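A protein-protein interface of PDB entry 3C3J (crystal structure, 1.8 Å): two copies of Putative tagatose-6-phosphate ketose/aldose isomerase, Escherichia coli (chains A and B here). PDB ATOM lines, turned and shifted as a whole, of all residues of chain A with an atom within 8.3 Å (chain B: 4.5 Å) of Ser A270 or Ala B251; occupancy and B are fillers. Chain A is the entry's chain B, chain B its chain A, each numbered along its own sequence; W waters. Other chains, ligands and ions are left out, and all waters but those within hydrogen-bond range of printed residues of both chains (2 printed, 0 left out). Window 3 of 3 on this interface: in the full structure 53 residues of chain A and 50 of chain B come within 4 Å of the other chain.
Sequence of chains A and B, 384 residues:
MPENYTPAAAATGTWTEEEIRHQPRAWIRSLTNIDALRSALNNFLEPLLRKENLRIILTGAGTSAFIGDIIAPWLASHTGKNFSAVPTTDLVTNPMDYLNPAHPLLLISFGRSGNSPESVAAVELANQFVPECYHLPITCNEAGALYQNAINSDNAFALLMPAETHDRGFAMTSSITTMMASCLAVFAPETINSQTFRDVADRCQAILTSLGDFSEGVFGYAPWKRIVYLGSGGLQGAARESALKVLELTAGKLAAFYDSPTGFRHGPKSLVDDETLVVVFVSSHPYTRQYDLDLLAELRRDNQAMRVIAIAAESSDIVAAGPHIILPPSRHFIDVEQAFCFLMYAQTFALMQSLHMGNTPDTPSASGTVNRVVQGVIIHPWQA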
ATOM      1  N   ARG A 226      -1.639  -0.616 -34.239  1.00  0.00           N
ATOM      2  CA  ARG A 226      -1.119  -0.987 -32.927  1.00  0.00           C
ATOM      3  C   ARG A 226      -2.182  -1.797 -32.197  1.00  0.00           C
ATOM      4  O   ARG A 226      -3.363  -1.460 -32.256  1.00  0.00           O
ATOM      5  CB  ARG A 226      -0.827   0.264 -32.110  1.00  0.00           C
ATOM      6  CG  ARG A 226       0.266   1.125 -32.668  1.00  0.00           C
ATOM      7  CD  ARG A 226       0.428   2.384 -31.867  1.00  0.00           C
ATOM      8  NE  ARG A 226       1.534   3.160 -32.393  1.00  0.00           N
ATOM      9  CZ  ARG A 226       2.034   4.239 -31.809  1.00  0.00           C
ATOM     10  NH1 ARG A 226       1.533   4.672 -30.662  1.00  0.00           N
ATOM     11  NH2 ARG A 226       3.036   4.884 -32.397  1.00  0.00           N
ATOM     12  N   PHE A 264      -0.369   0.002 -16.994  1.00  0.00           N
ATOM     13  CA  PHE A 264      -0.591   0.756 -18.237  1.00  0.00           C
ATOM     14  C   PHE A 264      -0.738   2.263 -17.983  1.00  0.00           C
ATOM     15  O   PHE A 264      -0.336   3.052 -18.789  1.00  0.00           O
ATOM     16  CB  PHE A 264      -1.844   0.215 -18.935  1.00  0.00           C
ATOM     17  CG  PHE A 264      -1.962   0.565 -20.403  1.00  0.00           C
ATOM     18  CD1 PHE A 264      -0.938   0.273 -21.300  1.00  0.00           C
ATOM     19  CD2 PHE A 264      -3.139   1.090 -20.897  1.00  0.00           C
ATOM     20  CE1 PHE A 264      -1.051   0.573 -22.649  1.00  0.00           C
ATOM     21  CE2 PHE A 264      -3.271   1.381 -22.264  1.00  0.00           C
ATOM     22  CZ  PHE A 264      -2.232   1.109 -23.137  1.00  0.00           C
ATOM     23  N   ARG A 265      -1.287   2.642 -16.839  1.00  0.00           N
ATOM     24  CA  ARG A 265      -1.495   4.039 -16.520  1.00  0.00           C
ATOM     25  C   ARG A 265      -0.205   4.820 -16.336  1.00  0.00           C
ATOM     26  O   ARG A 265      -0.197   6.016 -16.519  1.00  0.00           O
ATOM     27  CB  ARG A 265      -2.314   4.196 -15.236  1.00  0.00           C
ATOM     28  CG  ARG A 265      -3.748   3.822 -15.343  1.00  0.00           C
ATOM     29  CD  ARG A 265      -4.507   4.443 -14.192  1.00  0.00           C
ATOM     30  NE  ARG A 265      -5.920   4.102 -14.210  1.00  0.00           N
ATOM     31  CZ  ARG A 265      -6.433   3.005 -13.671  1.00  0.00           C
ATOM     32  NH1 ARG A 265      -5.634   2.132 -13.078  1.00  0.00           N
ATOM     33  NH2 ARG A 265      -7.759   2.796 -13.716  1.00  0.00           N
ATOM     34  N   HIS A 266       0.872   4.151 -15.963  1.00  0.00           N
ATOM     35  CA  HIS A 266       2.121   4.806 -15.576  1.00  0.00           C
ATOM     36  C   HIS A 266       3.078   5.089 -16.759  1.00  0.00           C
ATOM     37  O   HIS A 266       4.286   4.845 -16.696  1.00  0.00           O
ATOM     38  CB  HIS A 266       2.774   3.979 -14.479  1.00  0.00           C
ATOM     39  CG  HIS A 266       2.037   4.059 -13.181  1.00  0.00           C
ATOM     40  ND1 HIS A 266       1.026   3.189 -12.842  1.00  0.00           N
ATOM     41  CD2 HIS A 266       2.136   4.937 -12.156  1.00  0.00           C
ATOM     42  CE1 HIS A 266       0.547   3.516 -11.654  1.00  0.00           C
ATOM     43  NE2 HIS A 266       1.201   4.575 -11.219  1.00  0.00           N
ATOM     44  N   GLY A 267       2.521   5.623 -17.835  1.00  0.00           N
ATOM     45  CA  GLY A 267       3.294   5.970 -19.015  1.00  0.00           C
ATOM     46  C   GLY A 267       2.903   5.248 -20.295  1.00  0.00           C
ATOM     47  O   GLY A 267       2.760   5.900 -21.339  1.00  0.00           O
ATOM     48  N   PRO A 268       2.785   3.904 -20.264  1.00  0.00           N
ATOM     49  CA  PRO A 268       2.520   3.171 -21.516  1.00  0.00           C
ATOM     50  C   PRO A 268       1.245   3.554 -22.277  1.00  0.00           C
ATOM     51  O   PRO A 268       1.196   3.405 -23.497  1.00  0.00           O
ATOM     52  CB  PRO A 268       2.427   1.714 -21.052  1.00  0.00           C
ATOM     53  CG  PRO A 268       3.262   1.670 -19.828  1.00  0.00           C
ATOM     54  CD  PRO A 268       3.024   2.973 -19.144  1.00  0.00           C
ATOM     55  N   LYS A 269       0.262   4.080 -21.560  1.00  0.00           N
ATOM     56  CA  LYS A 269      -1.013   4.463 -22.133  1.00  0.00           C
ATOM     57  C   LYS A 269      -0.862   5.541 -23.187  1.00  0.00           C
ATOM     58  O   LYS A 269      -1.762   5.732 -23.996  1.00  0.00           O
ATOM     59  CB  LYS A 269      -1.931   4.987 -21.031  1.00  0.00           C
ATOM     60  CG  LYS A 269      -3.393   5.091 -21.394  1.00  0.00           C
ATOM     61  CD  LYS A 269      -4.032   6.200 -20.550  1.00  0.00           C
ATOM     62  CE  LYS A 269      -5.445   5.898 -20.184  1.00  0.00           C
ATOM     63  NZ  LYS A 269      -6.019   7.159 -19.628  1.00  0.00           N
ATOM     64  N   SER A 270       0.266   6.247 -23.169  1.00  0.00           N
ATOM     65  CA  SER A 270       0.563   7.237 -24.208  1.00  0.00           C
ATOM     66  C   SER A 270       0.611   6.601 -25.599  1.00  0.00           C
ATOM     67  O   SER A 270       0.403   7.289 -26.590  1.00  0.00           O
ATOM     68  CB  SER A 270       1.892   7.938 -23.925  1.00  0.00           C
ATOM     69  OG  SER A 270       2.896   6.973 -23.750  1.00  0.00           O
ATOM     70  N   LEU A 271       0.869   5.294 -25.677  1.00  0.00           N
ATOM     71  CA  LEU A 271       0.866   4.618 -26.984  1.00  0.00           C
ATOM     72  C   LEU A 271      -0.527   4.575 -27.675  1.00  0.00           C
ATOM     73  O   LEU A 271      -0.625   4.405 -28.901  1.00  0.00           O
ATOM     74  CB  LEU A 271       1.519   3.217 -26.864  1.00  0.00           C
ATOM     75  CG  LEU A 271       0.707   2.052 -26.319  1.00  0.00           C
ATOM     76  CD1 LEU A 271      -0.122   1.424 -27.446  1.00  0.00           C
ATOM     77  CD2 LEU A 271       1.615   1.015 -25.687  1.00  0.00           C
ATOM     78  N   VAL A 272      -1.603   4.699 -26.903  1.00  0.00           N
ATOM     79  CA  VAL A 272      -2.945   4.538 -27.451  1.00  0.00           C
ATOM     80  C   VAL A 272      -3.270   5.722 -28.378  1.00  0.00           C
ATOM     81  O   VAL A 272      -3.285   6.880 -27.951  1.00  0.00           O
ATOM     82  CB  VAL A 272      -4.021   4.442 -26.343  1.00  0.00           C
ATOM     83  CG1 VAL A 272      -5.410   4.480 -26.955  1.00  0.00           C
ATOM     84  CG2 VAL A 272      -3.809   3.198 -25.499  1.00  0.00           C
ATOM     85  N   ASP A 273      -3.501   5.409 -29.647  1.00  0.00           N
ATOM     86  CA  ASP A 273      -3.950   6.392 -30.639  1.00  0.00           C
ATOM     87  C   ASP A 273      -5.191   5.888 -31.396  1.00  0.00           C
ATOM     88  O   ASP A 273      -5.705   4.776 -31.151  1.00  0.00           O
ATOM     89  CB  ASP A 273      -2.792   6.750 -31.594  1.00  0.00           C
ATOM     90  CG  ASP A 273      -2.289   5.565 -32.438  1.00  0.00           C
ATOM     91  OD1 ASP A 273      -3.029   4.594 -32.680  1.00  0.00           O
ATOM     92  OD2 ASP A 273      -1.123   5.615 -32.906  1.00  0.00           O
ATOM     93  N   THR A 276      -5.278   2.382 -32.689  1.00  0.00           N
ATOM     94  CA  THR A 276      -4.958   1.353 -31.676  1.00  0.00           C
ATOM     95  C   THR A 276      -6.201   0.526 -31.227  1.00  0.00           C
ATOM     96  O   THR A 276      -7.267   1.075 -30.952  1.00  0.00           O
ATOM     97  CB  THR A 276      -4.315   1.979 -30.425  1.00  0.00           C
ATOM     98  OG1 THR A 276      -3.121   2.689 -30.778  1.00  0.00           O
ATOM     99  CG2 THR A 276      -3.976   0.886 -29.422  1.00  0.00           C
ATOM    100  N   ASP A 302     -11.773   7.758 -22.426  1.00  0.00           N
ATOM    101  CA  ASP A 302     -10.643   8.496 -23.017  1.00  0.00           C
ATOM    102  C   ASP A 302     -10.871   8.877 -24.469  1.00  0.00           C
ATOM    103  O   ASP A 302     -10.378   9.918 -24.896  1.00  0.00           O
ATOM    104  CB  ASP A 302      -9.336   7.682 -22.967  1.00  0.00           C
ATOM    105  CG  ASP A 302      -8.625   7.721 -21.598  1.00  0.00           C
ATOM    106  OD1 ASP A 302      -8.904   8.601 -20.741  1.00  0.00           O
ATOM    107  OD2 ASP A 302      -7.754   6.845 -21.394  1.00  0.00           O
ATOM    108  N   GLN A 304      -9.537   7.775 -27.132  1.00  0.00           N
ATOM    109  CA  GLN A 304      -8.301   7.811 -27.913  1.00  0.00           C
ATOM    110  C   GLN A 304      -8.204   6.634 -28.878  1.00  0.00           C
ATOM    111  O   GLN A 304      -7.791   6.803 -30.024  1.00  0.00           O
ATOM    112  CB  GLN A 304      -7.080   7.810 -26.985  1.00  0.00           C
ATOM    113  CG  GLN A 304      -6.938   9.075 -26.118  1.00  0.00           C
ATOM    114  CD  GLN A 304      -5.915   8.891 -24.955  1.00  0.00           C
ATOM    115  OE1 GLN A 304      -5.347   7.795 -24.757  1.00  0.00           O
ATOM    116  NE2 GLN A 304      -5.682   9.969 -24.191  1.00  0.00           N
ATOM    117  N   LEU B 247       8.419   6.784 -25.363  1.00  0.00           N
ATOM    118  CA  LEU B 247       6.998   6.684 -25.527  1.00  0.00           C
ATOM    119  C   LEU B 247       6.320   7.860 -24.824  1.00  0.00           C
ATOM    120  O   LEU B 247       5.515   8.555 -25.432  1.00  0.00           O
ATOM    121  CB  LEU B 247       6.529   5.355 -24.984  1.00  0.00           C
ATOM    122  CG  LEU B 247       5.199   4.868 -25.465  1.00  0.00           C
ATOM    123  CD1 LEU B 247       5.232   4.433 -26.941  1.00  0.00           C
ATOM    124  CD2 LEU B 247       4.821   3.707 -24.513  1.00  0.00           C
ATOM    125  N   GLU B 248       6.693   8.103 -23.570  1.00  0.00           N
ATOM    126  CA  GLU B 248       6.121   9.193 -22.779  1.00  0.00           C
ATOM    127  C   GLU B 248       6.351  10.550 -23.439  1.00  0.00           C
ATOM    128  O   GLU B 248       5.410  11.332 -23.669  1.00  0.00           O
ATOM    129  CB  GLU B 248       6.786   9.243 -21.405  1.00  0.00           C
ATOM    130  CG  GLU B 248       6.333   8.194 -20.489  1.00  0.00           C
ATOM    131  CD  GLU B 248       6.999   8.264 -19.150  1.00  0.00           C
ATOM    132  OE1 GLU B 248       8.142   8.772 -19.024  1.00  0.00           O
ATOM    133  OE2 GLU B 248       6.370   7.773 -18.202  1.00  0.00           O
ATOM    134  N   LEU B 249       7.616  10.847 -23.707  1.00  0.00           N
ATOM    135  CA  LEU B 249       7.985  12.205 -24.103  1.00  0.00           C
ATOM    136  C   LEU B 249       7.536  12.539 -25.538  1.00  0.00           C
ATOM    137  O   LEU B 249       7.350  13.724 -25.881  1.00  0.00           O
ATOM    138  CB  LEU B 249       9.482  12.433 -23.888  1.00  0.00           C
ATOM    139  CG  LEU B 249       9.920  12.428 -22.417  1.00  0.00           C
ATOM    140  CD1 LEU B 249      11.392  12.705 -22.297  1.00  0.00           C
ATOM    141  CD2 LEU B 249       9.115  13.423 -21.545  1.00  0.00           C
ATOM    142  N   THR B 250       7.342  11.507 -26.363  1.00  0.00           N
ATOM    143  CA  THR B 250       6.787  11.725 -27.713  1.00  0.00           C
ATOM    144  C   THR B 250       5.271  11.563 -27.788  1.00  0.00           C
ATOM    145  O   THR B 250       4.711  11.522 -28.893  1.00  0.00           O
ATOM    146  CB  THR B 250       7.434  10.831 -28.777  1.00  0.00           C
ATOM    147  OG1 THR B 250       7.027   9.461 -28.616  1.00  0.00           O
ATOM    148  CG2 THR B 250       8.983  10.986 -28.795  1.00  0.00           C
ATOM    149  N   ALA B 251       4.613  11.489 -26.630  1.00  0.00           N
ATOM    150  CA  ALA B 251       3.163  11.241 -26.534  1.00  0.00           C
ATOM    151  C   ALA B 251       2.732  10.070 -27.414  1.00  0.00           C
ATOM    152  O   ALA B 251       1.724  10.142 -28.117  1.00  0.00           O
ATOM    153  CB  ALA B 251       2.375  12.515 -26.915  1.00  0.00           C
ATOM    154  N   GLY B 252       3.525   9.006 -27.413  1.00  0.00           N
ATOM    155  CA  GLY B 252       3.186   7.829 -28.178  1.00  0.00           C
ATOM    156  C   GLY B 252       3.533   7.866 -29.644  1.00  0.00           C
ATOM    157  O   GLY B 252       3.390   6.851 -30.332  1.00  0.00           O
ATOM    158  N   LYS B 253       4.000   8.992 -30.158  1.00  0.00           N
ATOM    159  CA  LYS B 253       4.226   9.072 -31.600  1.00  0.00           C
ATOM    160  C   LYS B 253       5.320   8.144 -32.076  1.00  0.00           C
ATOM    161  O   LYS B 253       5.234   7.589 -33.164  1.00  0.00           O
ATOM    162  CB  LYS B 253       4.487  10.516 -32.028  1.00  0.00           C
ATOM    163  CG  LYS B 253       3.296  11.452 -31.742  1.00  0.00           C
ATOM    164  CD  LYS B 253       1.947  10.933 -32.277  1.00  0.00           C
ATOM    165  CE  LYS B 253       0.773  11.678 -31.630  1.00  0.00           C
ATOM    166  NZ  LYS B 253       0.848  11.657 -30.130  1.00  0.00           N
ATOM    167  N   ASN B 359       6.749  18.991 -29.160  1.00  0.00           N
ATOM    168  CA  ASN B 359       6.061  18.686 -27.913  1.00  0.00           C
ATOM    169  C   ASN B 359       6.690  19.453 -26.748  1.00  0.00           C
ATOM    170  O   ASN B 359       7.750  20.041 -26.892  1.00  0.00           O
ATOM    171  CB  ASN B 359       6.070  17.176 -27.659  1.00  0.00           C
ATOM    172  CG  ASN B 359       4.974  16.732 -26.703  1.00  0.00           C
ATOM    173  OD1 ASN B 359       4.101  17.522 -26.294  1.00  0.00           O
ATOM    174  ND2 ASN B 359       5.020  15.462 -26.323  1.00  0.00           N
HETATM  175  O   HOH W   1      -0.960   9.291 -26.838  1.00  0.00           O
HETATM  176  O   HOH W   2      -0.061   7.865 -29.718  1.00  0.00           O
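Among the printed residues, merely in contact across the chains: Ser A270 with Gly B252, Arg A226 with Lys B253, Gly A267 with Glu B248, Pro A268 with Leu B247, His A266 with Glu B248, Leu A271 with Leu B247 and Ser A270 with Glu B248.
No position is printed for both chains.
Ser A270 touches four residues of chain B.
Of the printed residues of chain A, Ala B251 touches Ser A270 (3.5 Å).
Of the printed residues of chain A, Glu B248 touches His A266 (3.9 Å), Gly A267 (3.7 Å) and Ser A270 (3.97 Å).
Printed residues of chain B within 4 Å of Gly A267: Glu B248.
Of the printed residues of chain B, Arg A226 touches Gly B252 and Lys B253.
Gln A304 touches none of the printed residues of chain B.
The nearest residue of chain A that does not touch Ala B251 is Leu A271 (5.4 Å).
The backbone carbonyl oxygen (O) of Leu B247 lies within hydrogen-bond range of the side-chain hydroxyl (OG) of Ser A270 (3.5 Å).
The backbone carbonyl oxygen of Ala B251 lies close to the backbone carbonyl oxygen of Ser A270, at 3.5 Å.
The backbone carbonyl oxygen of Gly B252 sits at hydrogen-bond distance from the guanidinium group of Arg A226.
Water W1 lies within hydrogen-bond range of O of Ser A270 and O of Ala B251.
Water W2 lies within hydrogen-bond range of O of Ser A270 (3.2 Å) and O of Ala B251 (3.3 Å).
OG1 of Thr B250 sits at hydrogen-bond distance from N of Lys B253, at 3.4 Å.
The backbone carbonyl oxygen (O) of Ala B251 lies within hydrogen-bond range of the side-chain amino group (NZ) of Lys B253.
The backbone carbonyl oxygen (O) of Leu A271 is in hydrogen-bond range of the guanidinium group (NH1) of Arg A226, at 2.8 Å.
The side-chain hydroxyl of Ser A270 sits at hydrogen-bond distance from the backbone carbonyl oxygen of Gly A267, 2.6 Å away.
O of Leu B247 lies within hydrogen-bond range of N of Gly B252.
NH1 of Arg A226 is in salt-bridge range of OD2 of Asp A273, at 3.6 Å.
Printed residues of chain B that touch a printed residue of chain A: Leu B247, Glu B248, Ala B251, Gly B252 and Lys B253.
Hydrophobic or aromatic side chains of chain B that line the printed part of chain A: Leu B247.
Among the printed residues, no Asp or Glu carboxylate lies within 4 Å of a Lys or Arg side-chain nitrogen of the other chain.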
